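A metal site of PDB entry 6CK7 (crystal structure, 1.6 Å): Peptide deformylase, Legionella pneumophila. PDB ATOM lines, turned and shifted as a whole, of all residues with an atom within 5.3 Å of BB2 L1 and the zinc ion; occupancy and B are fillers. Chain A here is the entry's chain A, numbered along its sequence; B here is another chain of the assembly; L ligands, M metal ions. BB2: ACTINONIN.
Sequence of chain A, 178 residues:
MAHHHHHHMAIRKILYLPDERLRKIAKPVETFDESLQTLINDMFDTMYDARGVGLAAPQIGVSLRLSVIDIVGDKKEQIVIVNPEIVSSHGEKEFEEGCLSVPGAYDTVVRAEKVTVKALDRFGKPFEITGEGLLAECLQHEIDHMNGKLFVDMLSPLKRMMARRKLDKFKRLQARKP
N1 of BB2 L1 lies within hydrogen-bond range of OE2 of Glu 142, 2.6 Å away. A nitrogen (N1) of BB2 L1 lies within hydrogen-bond range of the side-chain amide oxygen of Gln 59 (3.4 Å). The backbone NH (N) of Gly 98 is in hydrogen-bond range of an oxygen (O20) of BB2 L1. The backbone carbonyl oxygen of Gly 98 lies within hydrogen-bond range of a nitrogen (N14) of BB2 L1. N of Leu 100 sits close to O4 of BB2 L1. The backbone carbonyl oxygen (O) of Glu 96 of chain A is in hydrogen-bond range of an oxygen (O27) of BB2 L1 (2.9 Å). An oxygen (O13) of BB2 L1 is in hydrogen-bond range of the backbone NH (N) of Val 53 (2.9 Å). The backbone carbonyl oxygen (O) of Gly 54 sits close to a nitrogen (N1) of BB2 L1, 3.3 Å away. The backbone carbonyl oxygen of Glu 96 of chain B is in hydrogen-bond range of an oxygen (O27) of BB2 L2 (3.2 Å).
O27 of BB2 L2 sits close to O27 of BB2 L1, at 3.5 Å.
ND1 of His 141 is in hydrogen-bond range of OE2 of Glu 97, 2.7 Å away. NE2 of His 145 sits close to NE2 of Gln 59. SG of Cys 99 lies close to N of Ser 101, 3.3 Å away. SG of Cys 138 sits at hydrogen-bond distance from OE2 of Glu 142 (3.8 Å). The backbone NH (N) of Ala 56 sits at hydrogen-bond distance from the side-chain carboxylate (OE1) of Glu 142 (3.1 Å). The side-chain amide nitrogen (NE2) of Gln 59 lies within hydrogen-bond range of the side-chain hydroxyl (OG) of Ser 101 (3.0 Å). The side-chain carboxylate (OE1) of Glu 137 sits close to the side-chain carboxylate (OE1) of Glu 97 (2.6 Å). The side-chain hydroxyl (OH) of Tyr 106 of chain B lies within hydrogen-bond range of the backbone carbonyl oxygen (O) of Arg 51 (2.6 Å).
Residues that only touch BB2 L1: Gly 52 (3.4 Å), Glu 137 (3.5 Å), Cys 138 (3.6 Å), Tyr 106 of chain B (3.7 Å), Glu 97 (3.8 Å), Glu 96 of chain B (3.9 Å) and Tyr 106 of chain A (3.998 Å). Hydrophobic or aromatic side chains that line BB2 L1: Val 53, Leu 100, Tyr 106 of chain A, His 141, His 145 and Tyr 106 of chain B. Within 4 Å of BB2 L1: Gly 52, Val 53, Gly 54, Gln 59, Glu 96 of chain A, Glu 97, Gly 98, Cys 99, Leu 100, Tyr 106 of chain A, Glu 137, Cys 138, His 141, Glu 142, His 145, Glu 96 of chain B and Tyr 106 of chain B. Along chain A the residues within 4 Å of BB2 L1 span positions 52 to 145.
NE2 of Gln 59 touches the zinc ion, at 3.2 Å. Within 4 Å of the zinc ion: Gln 59, Cys 99, His 141 and His 145. Along chain A the residues within 4 Å of the zinc ion span positions 59 to 145.
A ring nitrogen (NE2) of His 141 binds the zinc ion, at 2.0 Å. A ring nitrogen (NE2) of His 145 is bound to the zinc ion (2.1 Å). The zinc ion is bound by O4 of BB2 L1 (2.1 Å). O2 of BB2 L1 is bound to the zinc ion, at 2.1 Å. The zinc ion is bound by SG of Cys 99 (2.3 Å).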
ATOM      1  N   ALA A  50      -5.281   6.750  25.603  1.00  0.00           N
ATOM      2  CA  ALA A  50      -5.590   5.454  26.181  1.00  0.00           C
ATOM      3  C   ALA A  50      -4.468   4.940  27.088  1.00  0.00           C
ATOM      4  O   ALA A  50      -4.542   3.791  27.542  1.00  0.00           O
ATOM      5  CB  ALA A  50      -5.850   4.440  25.059  1.00  0.00           C
ATOM      6  N   ARG A  51      -3.445   5.767  27.357  1.00  0.00           N
ATOM      7  CA  ARG A  51      -2.334   5.414  28.256  1.00  0.00           C
ATOM      8  C   ARG A  51      -1.510   4.237  27.731  1.00  0.00           C
ATOM      9  O   ARG A  51      -0.977   3.441  28.515  1.00  0.00           O
ATOM     10  CB  ARG A  51      -2.836   5.138  29.679  1.00  0.00           C
ATOM     11  CG  ARG A  51      -3.841   6.178  30.181  1.00  0.00           C
ATOM     12  CD  ARG A  51      -4.636   5.655  31.368  1.00  0.00           C
ATOM     13  NE  ARG A  51      -3.772   5.339  32.495  1.00  0.00           N
ATOM     14  CZ  ARG A  51      -4.154   5.391  33.774  1.00  0.00           C
ATOM     15  NH1 ARG A  51      -3.284   5.078  34.720  1.00  0.00           N
ATOM     16  NH2 ARG A  51      -5.388   5.763  34.082  1.00  0.00           N
ATOM     17  N   GLY A  52      -1.385   4.133  26.411  1.00  0.00           N
ATOM     18  CA  GLY A  52      -0.571   3.099  25.803  1.00  0.00           C
ATOM     19  C   GLY A  52       0.777   3.627  25.347  1.00  0.00           C
ATOM     20  O   GLY A  52       1.042   4.827  25.354  1.00  0.00           O
ATOM     21  N   VAL A  53       1.671   2.683  25.011  1.00  0.00           N
ATOM     22  CA  VAL A  53       2.951   3.036  24.414  1.00  0.00           C
ATOM     23  C   VAL A  53       3.044   2.599  22.961  1.00  0.00           C
ATOM     24  O   VAL A  53       4.089   2.816  22.321  1.00  0.00           O
ATOM     25  CB  VAL A  53       4.125   2.464  25.227  1.00  0.00           C
ATOM     26  CG1 VAL A  53       4.089   3.005  26.629  1.00  0.00           C
ATOM     27  CG2 VAL A  53       4.110   0.934  25.231  1.00  0.00           C
ATOM     28  N   GLY A  54       2.003   1.971  22.432  1.00  0.00           N
ATOM     29  CA  GLY A  54       1.926   1.671  21.013  1.00  0.00           C
ATOM     30  C   GLY A  54       0.475   1.523  20.630  1.00  0.00           C
ATOM     31  O   GLY A  54      -0.403   1.384  21.469  1.00  0.00           O
ATOM     32  N   LEU A  55       0.233   1.553  19.323  1.00  0.00           N
ATOM     33  CA  LEU A  55      -1.114   1.327  18.813  1.00  0.00           C
ATOM     34  C   LEU A  55      -0.982   0.914  17.350  1.00  0.00           C
ATOM     35  O   LEU A  55      -0.256   1.556  16.595  1.00  0.00           O
ATOM     36  CB  LEU A  55      -1.996   2.576  18.942  1.00  0.00           C
ATOM     37  CG  LEU A  55      -3.473   2.433  18.528  1.00  0.00           C
ATOM     38  CD1 LEU A  55      -4.250   1.661  19.567  1.00  0.00           C
ATOM     39  CD2 LEU A  55      -4.116   3.797  18.305  1.00  0.00           C
ATOM     40  N   ALA A  56      -1.703  -0.126  16.977  1.00  0.00           N
ATOM     41  CA  ALA A  56      -1.679  -0.635  15.617  1.00  0.00           C
ATOM     42  C   ALA A  56      -2.998  -0.298  14.940  1.00  0.00           C
ATOM     43  O   ALA A  56      -4.051  -0.305  15.592  1.00  0.00           O
ATOM     44  CB  ALA A  56      -1.425  -2.150  15.607  1.00  0.00           C
ATOM     45  N   GLN A  59      -6.375  -1.959  15.564  1.00  0.00           N
ATOM     46  CA  GLN A  59      -7.034  -1.721  16.843  1.00  0.00           C
ATOM     47  C   GLN A  59      -8.047  -0.588  16.785  1.00  0.00           C
ATOM     48  O   GLN A  59      -8.858  -0.485  17.712  1.00  0.00           O
ATOM     49  CB  GLN A  59      -6.010  -1.415  17.913  1.00  0.00           C
ATOM     50  CG  GLN A  59      -5.138  -2.594  18.253  1.00  0.00           C
ATOM     51  CD  GLN A  59      -4.145  -2.239  19.330  1.00  0.00           C
ATOM     52  OE1 GLN A  59      -3.057  -1.732  19.039  1.00  0.00           O
ATOM     53  NE2 GLN A  59      -4.528  -2.454  20.594  1.00  0.00           N
ATOM     54  N   GLU A  96       5.808  -8.785  31.393  1.00  0.00           N
ATOM     55  CA  GLU A  96       4.456  -8.527  31.885  1.00  0.00           C
ATOM     56  C   GLU A  96       3.775  -7.518  30.968  1.00  0.00           C
ATOM     57  O   GLU A  96       4.286  -6.402  30.808  1.00  0.00           O
ATOM     58  CB  GLU A  96       4.501  -7.997  33.325  1.00  0.00           C
ATOM     59  CG  GLU A  96       3.124  -7.571  33.851  1.00  0.00           C
ATOM     60  CD  GLU A  96       2.335  -8.748  34.369  1.00  0.00           C
ATOM     61  OE1 GLU A  96       2.906  -9.849  34.463  1.00  0.00           O
ATOM     62  OE2 GLU A  96       1.147  -8.569  34.710  1.00  0.00           O
ATOM     63  N   GLU A  97       2.635  -7.890  30.387  1.00  0.00           N
ATOM     64  CA  GLU A  97       2.098  -7.175  29.250  1.00  0.00           C
ATOM     65  C   GLU A  97       0.594  -6.982  29.359  1.00  0.00           C
ATOM     66  O   GLU A  97      -0.112  -7.856  29.870  1.00  0.00           O
ATOM     67  CB  GLU A  97       2.420  -7.935  27.963  1.00  0.00           C
ATOM     68  CG  GLU A  97       2.122  -7.233  26.673  1.00  0.00           C
ATOM     69  CD  GLU A  97       2.740  -7.973  25.510  1.00  0.00           C
ATOM     70  OE1 GLU A  97       3.970  -8.182  25.528  1.00  0.00           O
ATOM     71  OE2 GLU A  97       2.006  -8.374  24.619  1.00  0.00           O
ATOM     72  N   GLY A  98       0.109  -5.840  28.868  1.00  0.00           N
ATOM     73  CA  GLY A  98      -1.303  -5.632  28.596  1.00  0.00           C
ATOM     74  C   GLY A  98      -1.498  -5.130  27.175  1.00  0.00           C
ATOM     75  O   GLY A  98      -0.537  -4.899  26.451  1.00  0.00           O
ATOM     76  N   CYS A  99      -2.769  -4.986  26.806  1.00  0.00           N
ATOM     77  CA  CYS A  99      -3.134  -4.599  25.445  1.00  0.00           C
ATOM     78  C   CYS A  99      -4.337  -3.680  25.502  1.00  0.00           C
ATOM     79  O   CYS A  99      -5.291  -3.958  26.233  1.00  0.00           O
ATOM     80  CB  CYS A  99      -3.480  -5.846  24.598  1.00  0.00           C
ATOM     81  SG  CYS A  99      -3.935  -5.449  22.885  1.00  0.00           S
ATOM     82  N   LEU A 100      -4.301  -2.603  24.731  1.00  0.00           N
ATOM     83  CA  LEU A 100      -5.443  -1.686  24.696  1.00  0.00           C
ATOM     84  C   LEU A 100      -6.699  -2.349  24.150  1.00  0.00           C
ATOM     85  O   LEU A 100      -7.803  -1.866  24.416  1.00  0.00           O
ATOM     86  CB  LEU A 100      -5.088  -0.460  23.857  1.00  0.00           C
ATOM     87  CG  LEU A 100      -3.991   0.439  24.434  1.00  0.00           C
ATOM     88  CD1 LEU A 100      -3.702   1.612  23.525  1.00  0.00           C
ATOM     89  CD2 LEU A 100      -4.350   0.903  25.829  1.00  0.00           C
ATOM     90  N   SER A 101      -6.563  -3.459  23.419  1.00  0.00           N
ATOM     91  CA  SER A 101      -7.698  -4.176  22.864  1.00  0.00           C
ATOM     92  C   SER A 101      -8.145  -5.325  23.756  1.00  0.00           C
ATOM     93  O   SER A 101      -9.089  -6.040  23.402  1.00  0.00           O
ATOM     94  CB  SER A 101      -7.379  -4.674  21.452  1.00  0.00           C
ATOM     95  OG  SER A 101      -7.286  -3.574  20.552  1.00  0.00           O
ATOM     96  N   TYR A 106      -3.741  -8.623  32.203  1.00  0.00           N
ATOM     97  CA  TYR A 106      -2.295  -8.515  32.317  1.00  0.00           C
ATOM     98  C   TYR A 106      -1.722  -9.905  32.514  1.00  0.00           C
ATOM     99  O   TYR A 106      -2.208 -10.652  33.356  1.00  0.00           O
ATOM    100  CB  TYR A 106      -1.877  -7.615  33.501  1.00  0.00           C
ATOM    101  CG  TYR A 106      -2.434  -6.241  33.360  1.00  0.00           C
ATOM    102  CD1 TYR A 106      -1.892  -5.338  32.442  1.00  0.00           C
ATOM    103  CD2 TYR A 106      -3.505  -5.823  34.139  1.00  0.00           C
ATOM    104  CE1 TYR A 106      -2.402  -4.064  32.304  1.00  0.00           C
ATOM    105  CE2 TYR A 106      -4.032  -4.539  33.998  1.00  0.00           C
ATOM    106  CZ  TYR A 106      -3.472  -3.666  33.075  1.00  0.00           C
ATOM    107  OH  TYR A 106      -3.971  -2.403  32.902  1.00  0.00           O
ATOM    108  N   LEU A 134      11.579  -3.061  26.506  1.00  0.00           N
ATOM    109  CA  LEU A 134      10.229  -2.644  26.169  1.00  0.00           C
ATOM    110  C   LEU A 134      10.052  -2.372  24.675  1.00  0.00           C
ATOM    111  O   LEU A 134       9.012  -2.710  24.102  1.00  0.00           O
ATOM    112  CB  LEU A 134       9.831  -1.405  26.964  1.00  0.00           C
ATOM    113  CG  LEU A 134       9.546  -1.550  28.454  1.00  0.00           C
ATOM    114  CD1 LEU A 134       8.952  -0.242  28.971  1.00  0.00           C
ATOM    115  CD2 LEU A 134       8.606  -2.710  28.726  1.00  0.00           C
ATOM    116  N   GLU A 137       9.669  -5.635  22.922  1.00  0.00           N
ATOM    117  CA  GLU A 137       8.369  -6.197  23.246  1.00  0.00           C
ATOM    118  C   GLU A 137       7.276  -5.497  22.469  1.00  0.00           C
ATOM    119  O   GLU A 137       6.408  -6.129  21.869  1.00  0.00           O
ATOM    120  CB  GLU A 137       8.120  -6.094  24.757  1.00  0.00           C
ATOM    121  CG  GLU A 137       6.789  -6.657  25.194  1.00  0.00           C
ATOM    122  CD  GLU A 137       6.389  -6.201  26.593  1.00  0.00           C
ATOM    123  OE1 GLU A 137       5.385  -6.722  27.116  1.00  0.00           O
ATOM    124  OE2 GLU A 137       7.074  -5.332  27.158  1.00  0.00           O
ATOM    125  N   CYS A 138       7.346  -4.162  22.431  1.00  0.00           N
ATOM    126  CA  CYS A 138       6.311  -3.374  21.758  1.00  0.00           C
ATOM    127  C   CYS A 138       6.313  -3.639  20.257  1.00  0.00           C
ATOM    128  O   CYS A 138       5.261  -3.809  19.643  1.00  0.00           O
ATOM    129  CB  CYS A 138       6.545  -1.891  22.037  1.00  0.00           C
ATOM    130  SG  CYS A 138       5.206  -0.863  21.443  1.00  0.00           S
ATOM    131  N   HIS A 141       4.693  -6.906  19.669  1.00  0.00           N
ATOM    132  CA  HIS A 141       3.271  -6.798  19.982  1.00  0.00           C
ATOM    133  C   HIS A 141       2.506  -6.090  18.855  1.00  0.00           C
ATOM    134  O   HIS A 141       1.421  -6.542  18.448  1.00  0.00           O
ATOM    135  CB  HIS A 141       3.113  -6.061  21.323  1.00  0.00           C
ATOM    136  CG  HIS A 141       1.689  -5.858  21.776  1.00  0.00           C
ATOM    137  ND1 HIS A 141       1.166  -6.520  22.866  1.00  0.00           N
ATOM    138  CD2 HIS A 141       0.709  -5.037  21.320  1.00  0.00           C
ATOM    139  CE1 HIS A 141      -0.076  -6.110  23.072  1.00  0.00           C
ATOM    140  NE2 HIS A 141      -0.394  -5.226  22.132  1.00  0.00           N
ATOM    141  N   GLU A 142       3.067  -5.009  18.325  1.00  0.00           N
ATOM    142  CA  GLU A 142       2.371  -4.260  17.287  1.00  0.00           C
ATOM    143  C   GLU A 142       2.320  -5.043  15.984  1.00  0.00           C
ATOM    144  O   GLU A 142       1.297  -5.026  15.284  1.00  0.00           O
ATOM    145  CB  GLU A 142       3.034  -2.905  17.042  1.00  0.00           C
ATOM    146  CG  GLU A 142       3.088  -1.977  18.266  1.00  0.00           C
ATOM    147  CD  GLU A 142       1.748  -1.751  18.933  1.00  0.00           C
ATOM    148  OE1 GLU A 142       0.714  -1.713  18.226  1.00  0.00           O
ATOM    149  OE2 GLU A 142       1.737  -1.592  20.171  1.00  0.00           O
ATOM    150  N   HIS A 145      -0.436  -7.623  16.027  1.00  0.00           N
ATOM    151  CA  HIS A 145      -1.735  -7.035  15.698  1.00  0.00           C
ATOM    152  C   HIS A 145      -1.954  -6.960  14.189  1.00  0.00           C
ATOM    153  O   HIS A 145      -3.085  -7.130  13.704  1.00  0.00           O
ATOM    154  CB  HIS A 145      -1.860  -5.623  16.290  1.00  0.00           C
ATOM    155  CG  HIS A 145      -2.341  -5.564  17.705  1.00  0.00           C
ATOM    156  ND1 HIS A 145      -3.562  -6.065  18.117  1.00  0.00           N
ATOM    157  CD2 HIS A 145      -1.776  -5.014  18.806  1.00  0.00           C
ATOM    158  CE1 HIS A 145      -3.720  -5.843  19.414  1.00  0.00           C
ATOM    159  NE2 HIS A 145      -2.648  -5.205  19.856  1.00  0.00           N
ATOM    160  N   GLU B  96       8.642  -2.249  36.612  1.00  0.00           N
ATOM    161  CA  GLU B  96       8.022  -1.321  35.675  1.00  0.00           C
ATOM    162  C   GLU B  96       6.600  -1.072  36.136  1.00  0.00           C
ATOM    163  O   GLU B  96       5.816  -2.024  36.265  1.00  0.00           O
ATOM    164  CB  GLU B  96       8.039  -1.897  34.263  1.00  0.00           C
ATOM    165  CG  GLU B  96       7.277  -1.059  33.235  1.00  0.00           C
ATOM    166  CD  GLU B  96       8.044   0.164  32.807  1.00  0.00           C
ATOM    167  OE1 GLU B  96       7.494   0.954  32.025  1.00  0.00           O
ATOM    168  OE2 GLU B  96       9.216   0.318  33.198  1.00  0.00           O
ATOM    169  N   TYR B 106       4.819   5.680  32.803  1.00  0.00           N
ATOM    170  CA  TYR B 106       5.346   4.369  33.140  1.00  0.00           C
ATOM    171  C   TYR B 106       6.834   4.531  33.406  1.00  0.00           C
ATOM    172  O   TYR B 106       7.539   5.145  32.608  1.00  0.00           O
ATOM    173  CB  TYR B 106       5.121   3.351  31.996  1.00  0.00           C
ATOM    174  CG  TYR B 106       3.669   3.180  31.695  1.00  0.00           C
ATOM    175  CD1 TYR B 106       2.850   2.469  32.559  1.00  0.00           C
ATOM    176  CD2 TYR B 106       3.100   3.785  30.581  1.00  0.00           C
ATOM    177  CE1 TYR B 106       1.493   2.335  32.309  1.00  0.00           C
ATOM    178  CE2 TYR B 106       1.744   3.671  30.317  1.00  0.00           C
ATOM    179  CZ  TYR B 106       0.948   2.942  31.194  1.00  0.00           C
ATOM    180  OH  TYR B 106      -0.396   2.799  30.969  1.00  0.00           O
HETATM  181  C5  BB2 L   1      -0.476  -1.060  23.571  1.00  0.00           C
HETATM  182  C3  BB2 L   1      -1.138  -1.922  22.525  1.00  0.00           C
HETATM  183  O4  BB2 L   1      -2.124  -2.580  22.795  1.00  0.00           O
HETATM  184  N1  BB2 L   1      -0.603  -1.931  21.322  1.00  0.00           N
HETATM  185  O2  BB2 L   1      -1.237  -2.921  20.579  1.00  0.00           O
HETATM  186  C6  BB2 L   1       0.341  -1.927  24.517  1.00  0.00           C
HETATM  187  C12 BB2 L   1       0.474  -1.165  25.809  1.00  0.00           C
HETATM  188  O13 BB2 L   1       0.771   0.020  25.858  1.00  0.00           O
HETATM  189  C7  BB2 L   1       1.718  -2.296  23.979  1.00  0.00           C
HETATM  190  C8  BB2 L   1       2.277  -3.425  24.858  1.00  0.00           C
HETATM  191  C9  BB2 L   1       3.629  -3.992  24.485  1.00  0.00           C
HETATM  192  C10 BB2 L   1       4.795  -3.179  25.044  1.00  0.00           C
HETATM  193  C11 BB2 L   1       4.618  -2.941  26.522  1.00  0.00           C
HETATM  194  N14 BB2 L   1       0.218  -1.893  26.897  1.00  0.00           N
HETATM  195  C15 BB2 L   1       0.407  -1.345  28.229  1.00  0.00           C
HETATM  196  C16 BB2 L   1      -0.898  -1.473  28.997  1.00  0.00           C
HETATM  197  C18 BB2 L   1      -0.756  -0.938  30.432  1.00  0.00           C
HETATM  198  C17 BB2 L   1      -2.073  -0.804  28.257  1.00  0.00           C
HETATM  199  C19 BB2 L   1       1.507  -2.098  28.918  1.00  0.00           C
HETATM  200  O20 BB2 L   1       1.450  -3.311  28.953  1.00  0.00           O
HETATM  201  N21 BB2 L   1       2.510  -1.364  29.406  1.00  0.00           N
HETATM  202  C22 BB2 L   1       3.718  -1.980  29.986  1.00  0.00           C
HETATM  203  C23 BB2 L   1       2.613   0.085  29.358  1.00  0.00           C
HETATM  204  C24 BB2 L   1       4.105   0.366  29.375  1.00  0.00           C
HETATM  205  C25 BB2 L   1       4.742  -0.852  30.020  1.00  0.00           C
HETATM  206  C26 BB2 L   1       3.361  -2.345  31.418  1.00  0.00           C
HETATM  207  O27 BB2 L   1       3.234  -3.762  31.516  1.00  0.00           O
HETATM  208  C5  BB2 L   2      -3.032   0.867  40.526  1.00  0.00           C
HETATM  209  C3  BB2 L   2      -2.891   2.043  41.448  1.00  0.00           C
HETATM  210  O4  BB2 L   2      -2.591   3.148  41.031  1.00  0.00           O
HETATM  211  N1  BB2 L   2      -3.116   1.865  42.732  1.00  0.00           N
HETATM  212  O2  BB2 L   2      -2.793   2.983  43.473  1.00  0.00           O
HETATM  213  C6  BB2 L   2      -1.660   0.458  40.017  1.00  0.00           C
HETATM  214  C12 BB2 L   2      -1.821  -0.256  38.709  1.00  0.00           C
HETATM  215  O13 BB2 L   2      -2.709  -1.103  38.554  1.00  0.00           O
HETATM  216  C7  BB2 L   2      -0.932  -0.452  41.003  1.00  0.00           C
HETATM  217  C8  BB2 L   2       0.535  -0.540  40.554  1.00  0.00           C
HETATM  218  C9  BB2 L   2       1.452  -1.269  41.526  1.00  0.00           C
HETATM  219  C10 BB2 L   2       1.524  -2.757  41.215  1.00  0.00           C
HETATM  220  C11 BB2 L   2       1.735  -2.958  39.730  1.00  0.00           C
HETATM  221  N14 BB2 L   2      -0.942   0.060  37.781  1.00  0.00           N
HETATM  222  C15 BB2 L   2      -0.923  -0.619  36.501  1.00  0.00           C
HETATM  223  C16 BB2 L   2      -1.101   0.421  35.391  1.00  0.00           C
HETATM  224  C18 BB2 L   2      -1.002  -0.245  34.021  1.00  0.00           C
HETATM  225  C17 BB2 L   2      -2.400   1.203  35.482  1.00  0.00           C
HETATM  226  C19 BB2 L   2       0.374  -1.358  36.358  1.00  0.00           C
HETATM  227  O20 BB2 L   2       1.455  -0.777  36.528  1.00  0.00           O
HETATM  228  N21 BB2 L   2       0.286  -2.662  36.103  1.00  0.00           N
HETATM  229  C22 BB2 L   2       1.487  -3.487  36.037  1.00  0.00           C
HETATM  230  C23 BB2 L   2      -0.943  -3.440  35.922  1.00  0.00           C
HETATM  231  C24 BB2 L   2      -0.531  -4.861  36.285  1.00  0.00           C
HETATM  232  C25 BB2 L   2       0.982  -4.924  36.162  1.00  0.00           C
HETATM  233  C26 BB2 L   2       2.032  -3.298  34.619  1.00  0.00           C
HETATM  234  O27 BB2 L   2       3.068  -2.306  34.661  1.00  0.00           O
HETATM  235 ZN    ZN M   1      -2.209  -4.416  21.747  1.00  0.00          ZN
